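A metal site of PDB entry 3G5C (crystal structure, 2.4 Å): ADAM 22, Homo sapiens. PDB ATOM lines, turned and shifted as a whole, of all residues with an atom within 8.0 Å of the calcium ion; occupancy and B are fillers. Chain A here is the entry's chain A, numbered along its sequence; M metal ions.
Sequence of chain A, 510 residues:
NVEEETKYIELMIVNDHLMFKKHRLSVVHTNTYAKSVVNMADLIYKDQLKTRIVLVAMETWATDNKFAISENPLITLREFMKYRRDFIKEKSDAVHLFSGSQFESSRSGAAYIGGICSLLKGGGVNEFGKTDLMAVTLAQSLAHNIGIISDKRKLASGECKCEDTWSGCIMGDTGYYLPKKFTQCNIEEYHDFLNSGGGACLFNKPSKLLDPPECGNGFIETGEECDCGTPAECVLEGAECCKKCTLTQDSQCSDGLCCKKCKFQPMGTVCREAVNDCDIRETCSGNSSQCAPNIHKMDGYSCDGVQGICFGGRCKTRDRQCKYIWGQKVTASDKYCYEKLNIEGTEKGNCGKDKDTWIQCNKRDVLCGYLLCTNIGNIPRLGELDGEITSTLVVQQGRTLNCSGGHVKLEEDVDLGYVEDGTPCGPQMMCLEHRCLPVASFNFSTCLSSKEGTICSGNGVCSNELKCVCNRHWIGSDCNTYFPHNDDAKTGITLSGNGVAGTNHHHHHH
The side-chain carboxylate of Asp 227 lies close to the backbone NH of Gly 216, at 3.4 Å.
The side-chain carboxylate (OD1) of Asp 227 sits at hydrogen-bond distance from the backbone NH (N) of Gly 218.
The backbone NH of Phe 219 lies close to the side-chain amide oxygen of Asn 217 (2.9 Å).
The side-chain sulfur of Cys 215 is disulfide-bonded to the side-chain sulfur of Cys 245 (2.0 Å).
OE1 of Glu 224 sits close to O of Phe 219 (2.6 Å).
Residues that only touch the calcium ion: Cys 215 (3.5 Å) and Gly 216 (3.6 Å).
Eight residues have an atom within 4 Å of the calcium ion: Glu 214, Cys 215, Gly 216, Asn 217, Phe 219, Glu 221, Glu 224 and Asp 227.
Along chain A the residues within 4 Å of the calcium ion span positions 214 to 227.
The nearest printed residue that does not touch the calcium ion is Cys 245 (4.6 Å).
The calcium ion is bound by OD2 of Asp 227, O of Glu 214, OD1 of Asn 217, OE1 of Glu 221, OE1 of Glu 224 and OE2 of Glu 224.
The calcium ion has six donor atoms within binding distance.
Slightly farther from the calcium ion lies O of Phe 219 (2.9 Å).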
ATOM      1  N   SER A 207      27.912 -25.789 -16.785  1.00  0.00           N
ATOM      2  CA  SER A 207      28.361 -24.405 -16.929  1.00  0.00           C
ATOM      3  C   SER A 207      29.687 -24.326 -17.683  1.00  0.00           C
ATOM      4  O   SER A 207      29.731 -23.861 -18.827  1.00  0.00           O
ATOM      5  CB  SER A 207      28.480 -23.763 -15.553  1.00  0.00           C
ATOM      6  OG  SER A 207      29.242 -24.579 -14.681  1.00  0.00           O
ATOM      7  N   LEU A 209      31.959 -25.866 -19.787  1.00  0.00           N
ATOM      8  CA  LEU A 209      32.313 -26.894 -20.763  1.00  0.00           C
ATOM      9  C   LEU A 209      33.837 -26.789 -20.952  1.00  0.00           C
ATOM     10  O   LEU A 209      34.414 -25.714 -20.958  1.00  0.00           O
ATOM     11  CB  LEU A 209      31.475 -26.729 -22.033  1.00  0.00           C
ATOM     12  CG  LEU A 209      30.182 -25.942 -21.893  1.00  0.00           C
ATOM     13  CD1 LEU A 209      29.437 -25.883 -23.225  1.00  0.00           C
ATOM     14  CD2 LEU A 209      29.302 -26.542 -20.811  1.00  0.00           C
ATOM     15  N   PRO A 212      36.925 -23.047 -23.918  1.00  0.00           N
ATOM     16  CA  PRO A 212      36.830 -21.584 -23.592  1.00  0.00           C
ATOM     17  C   PRO A 212      35.461 -20.970 -23.913  1.00  0.00           C
ATOM     18  O   PRO A 212      34.876 -21.270 -24.951  1.00  0.00           O
ATOM     19  CB  PRO A 212      38.007 -21.048 -24.362  1.00  0.00           C
ATOM     20  CG  PRO A 212      39.032 -21.948 -23.777  1.00  0.00           C
ATOM     21  CD  PRO A 212      38.344 -23.291 -23.609  1.00  0.00           C
ATOM     22  N   PRO A 213      34.944 -20.101 -23.001  1.00  0.00           N
ATOM     23  CA  PRO A 213      33.639 -19.456 -23.126  1.00  0.00           C
ATOM     24  C   PRO A 213      33.355 -18.797 -24.468  1.00  0.00           C
ATOM     25  O   PRO A 213      34.246 -18.199 -25.075  1.00  0.00           O
ATOM     26  CB  PRO A 213      33.632 -18.465 -21.967  1.00  0.00           C
ATOM     27  CG  PRO A 213      34.384 -19.219 -20.921  1.00  0.00           C
ATOM     28  CD  PRO A 213      35.555 -19.774 -21.695  1.00  0.00           C
ATOM     29  N   GLU A 214      32.112 -18.914 -24.916  1.00  0.00           N
ATOM     30  CA  GLU A 214      31.647 -18.306 -26.164  1.00  0.00           C
ATOM     31  C   GLU A 214      30.203 -17.855 -25.957  1.00  0.00           C
ATOM     32  O   GLU A 214      29.313 -18.669 -25.746  1.00  0.00           O
ATOM     33  CB  GLU A 214      31.751 -19.345 -27.284  1.00  0.00           C
ATOM     34  CG  GLU A 214      31.465 -18.808 -28.674  1.00  0.00           C
ATOM     35  CD  GLU A 214      29.994 -18.898 -29.042  1.00  0.00           C
ATOM     36  OE1 GLU A 214      29.635 -18.454 -30.151  1.00  0.00           O
ATOM     37  OE2 GLU A 214      29.200 -19.419 -28.227  1.00  0.00           O
ATOM     38  N   CYS A 215      29.996 -16.540 -26.012  1.00  0.00           N
ATOM     39  CA  CYS A 215      28.678 -15.960 -25.773  1.00  0.00           C
ATOM     40  C   CYS A 215      27.692 -16.239 -26.910  1.00  0.00           C
ATOM     41  O   CYS A 215      27.889 -15.797 -28.042  1.00  0.00           O
ATOM     42  CB  CYS A 215      28.773 -14.447 -25.536  1.00  0.00           C
ATOM     43  SG  CYS A 215      27.095 -13.783 -25.245  1.00  0.00           S
ATOM     44  N   GLY A 216      26.641 -16.997 -26.586  1.00  0.00           N
ATOM     45  CA  GLY A 216      25.600 -17.303 -27.553  1.00  0.00           C
ATOM     46  C   GLY A 216      25.458 -18.774 -27.909  1.00  0.00           C
ATOM     47  O   GLY A 216      24.902 -19.115 -28.956  1.00  0.00           O
ATOM     48  N   ASN A 217      25.965 -19.655 -27.042  1.00  0.00           N
ATOM     49  CA  ASN A 217      25.823 -21.102 -27.239  1.00  0.00           C
ATOM     50  C   ASN A 217      24.687 -21.689 -26.397  1.00  0.00           C
ATOM     51  O   ASN A 217      24.303 -22.846 -26.574  1.00  0.00           O
ATOM     52  CB  ASN A 217      27.139 -21.808 -26.903  1.00  0.00           C
ATOM     53  CG  ASN A 217      27.606 -21.504 -25.506  1.00  0.00           C
ATOM     54  OD1 ASN A 217      26.929 -20.811 -24.760  1.00  0.00           O
ATOM     55  ND2 ASN A 217      28.767 -22.032 -25.139  1.00  0.00           N
ATOM     56  N   GLY A 218      24.150 -20.880 -25.485  1.00  0.00           N
ATOM     57  CA  GLY A 218      23.062 -21.293 -24.609  1.00  0.00           C
ATOM     58  C   GLY A 218      23.514 -21.830 -23.264  1.00  0.00           C
ATOM     59  O   GLY A 218      22.715 -22.350 -22.494  1.00  0.00           O
ATOM     60  N   PHE A 219      24.814 -21.694 -22.997  1.00  0.00           N
ATOM     61  CA  PHE A 219      25.418 -22.186 -21.757  1.00  0.00           C
ATOM     62  C   PHE A 219      26.101 -21.049 -21.018  1.00  0.00           C
ATOM     63  O   PHE A 219      26.956 -20.366 -21.578  1.00  0.00           O
ATOM     64  CB  PHE A 219      26.447 -23.265 -22.063  1.00  0.00           C
ATOM     65  CG  PHE A 219      25.872 -24.478 -22.688  1.00  0.00           C
ATOM     66  CD1 PHE A 219      25.368 -24.443 -23.985  1.00  0.00           C
ATOM     67  CD2 PHE A 219      25.817 -25.674 -21.977  1.00  0.00           C
ATOM     68  CE1 PHE A 219      24.801 -25.574 -24.567  1.00  0.00           C
ATOM     69  CE2 PHE A 219      25.256 -26.818 -22.549  1.00  0.00           C
ATOM     70  CZ  PHE A 219      24.753 -26.764 -23.842  1.00  0.00           C
ATOM     71  N   ILE A 220      25.720 -20.850 -19.757  1.00  0.00           N
ATOM     72  CA  ILE A 220      26.314 -19.800 -18.929  1.00  0.00           C
ATOM     73  C   ILE A 220      27.679 -20.254 -18.411  1.00  0.00           C
ATOM     74  O   ILE A 220      27.788 -21.042 -17.473  1.00  0.00           O
ATOM     75  CB  ILE A 220      25.407 -19.417 -17.770  1.00  0.00           C
ATOM     76  CG1 ILE A 220      24.042 -18.975 -18.323  1.00  0.00           C
ATOM     77  CG2 ILE A 220      26.045 -18.275 -16.993  1.00  0.00           C
ATOM     78  CD1 ILE A 220      22.947 -18.876 -17.298  1.00  0.00           C
ATOM     79  N   GLU A 221      28.734 -19.739 -19.059  1.00  0.00           N
ATOM     80  CA  GLU A 221      30.110 -20.077 -18.732  1.00  0.00           C
ATOM     81  C   GLU A 221      30.724 -19.021 -17.807  1.00  0.00           C
ATOM     82  O   GLU A 221      30.004 -18.173 -17.264  1.00  0.00           O
ATOM     83  CB  GLU A 221      30.905 -20.192 -20.031  1.00  0.00           C
ATOM     84  CG  GLU A 221      30.372 -21.300 -20.935  1.00  0.00           C
ATOM     85  CD  GLU A 221      30.624 -21.084 -22.433  1.00  0.00           C
ATOM     86  OE1 GLU A 221      29.977 -20.178 -23.022  1.00  0.00           O
ATOM     87  OE2 GLU A 221      31.458 -21.818 -23.005  1.00  0.00           O
ATOM     88  N   THR A 222      32.040 -19.086 -17.610  1.00  0.00           N
ATOM     89  CA  THR A 222      32.745 -18.110 -16.764  1.00  0.00           C
ATOM     90  C   THR A 222      32.884 -16.757 -17.464  1.00  0.00           C
ATOM     91  O   THR A 222      33.371 -16.684 -18.604  1.00  0.00           O
ATOM     92  CB  THR A 222      34.145 -18.598 -16.328  1.00  0.00           C
ATOM     93  OG1 THR A 222      34.780 -19.276 -17.426  1.00  0.00           O
ATOM     94  CG2 THR A 222      34.043 -19.516 -15.128  1.00  0.00           C
ATOM     95  N   GLU A 224      30.315 -14.670 -18.263  1.00  0.00           N
ATOM     96  CA  GLU A 224      28.974 -14.288 -18.699  1.00  0.00           C
ATOM     97  C   GLU A 224      27.911 -14.582 -17.635  1.00  0.00           C
ATOM     98  O   GLU A 224      27.969 -15.595 -16.950  1.00  0.00           O
ATOM     99  CB  GLU A 224      28.642 -15.036 -20.006  1.00  0.00           C
ATOM    100  CG  GLU A 224      28.778 -16.553 -19.901  1.00  0.00           C
ATOM    101  CD  GLU A 224      28.723 -17.270 -21.246  1.00  0.00           C
ATOM    102  OE1 GLU A 224      28.744 -18.512 -21.271  1.00  0.00           O
ATOM    103  OE2 GLU A 224      28.657 -16.574 -22.286  1.00  0.00           O
ATOM    104  N   CYS A 226      24.252 -14.063 -18.198  1.00  0.00           N
ATOM    105  CA  CYS A 226      23.165 -14.795 -18.835  1.00  0.00           C
ATOM    106  C   CYS A 226      23.616 -15.360 -20.179  1.00  0.00           C
ATOM    107  O   CYS A 226      24.759 -15.152 -20.606  1.00  0.00           O
ATOM    108  CB  CYS A 226      21.977 -13.863 -19.073  1.00  0.00           C
ATOM    109  SG  CYS A 226      22.367 -12.462 -20.178  1.00  0.00           S
ATOM    110  N   ASP A 227      22.700 -16.079 -20.834  1.00  0.00           N
ATOM    111  CA  ASP A 227      22.916 -16.635 -22.148  1.00  0.00           C
ATOM    112  C   ASP A 227      21.628 -17.285 -22.639  1.00  0.00           C
ATOM    113  O   ASP A 227      21.186 -18.294 -22.084  1.00  0.00           O
ATOM    114  CB  ASP A 227      24.039 -17.696 -22.084  1.00  0.00           C
ATOM    115  CG  ASP A 227      24.668 -17.963 -23.437  1.00  0.00           C
ATOM    116  OD1 ASP A 227      23.939 -17.931 -24.440  1.00  0.00           O
ATOM    117  OD2 ASP A 227      25.895 -18.210 -23.489  1.00  0.00           O
ATOM    118  N   CYS A 228      21.006 -16.676 -23.631  1.00  0.00           N
ATOM    119  CA  CYS A 228      19.857 -17.280 -24.309  1.00  0.00           C
ATOM    120  C   CYS A 228      20.424 -18.216 -25.390  1.00  0.00           C
ATOM    121  O   CYS A 228      21.638 -18.338 -25.530  1.00  0.00           O
ATOM    122  CB  CYS A 228      18.978 -16.179 -24.915  1.00  0.00           C
ATOM    123  SG  CYS A 228      19.791 -15.027 -26.049  1.00  0.00           S
ATOM    124  N   GLY A 229      19.540 -18.882 -26.142  1.00  0.00           N
ATOM    125  CA  GLY A 229      19.980 -19.805 -27.193  1.00  0.00           C
ATOM    126  C   GLY A 229      20.890 -19.132 -28.205  1.00  0.00           C
ATOM    127  O   GLY A 229      22.111 -19.111 -28.037  1.00  0.00           O
ATOM    128  N   CYS A 245      25.368 -11.338 -23.250  1.00  0.00           N
ATOM    129  CA  CYS A 245      25.609 -12.171 -22.072  1.00  0.00           C
ATOM    130  C   CYS A 245      25.610 -11.383 -20.755  1.00  0.00           C
ATOM    131  O   CYS A 245      26.294 -11.741 -19.795  1.00  0.00           O
ATOM    132  CB  CYS A 245      26.922 -12.966 -22.271  1.00  0.00           C
ATOM    133  SG  CYS A 245      26.643 -14.406 -23.365  1.00  0.00           S
HETATM  134 CA    CA M   1      28.010 -18.818 -23.837  1.00  0.00          CA
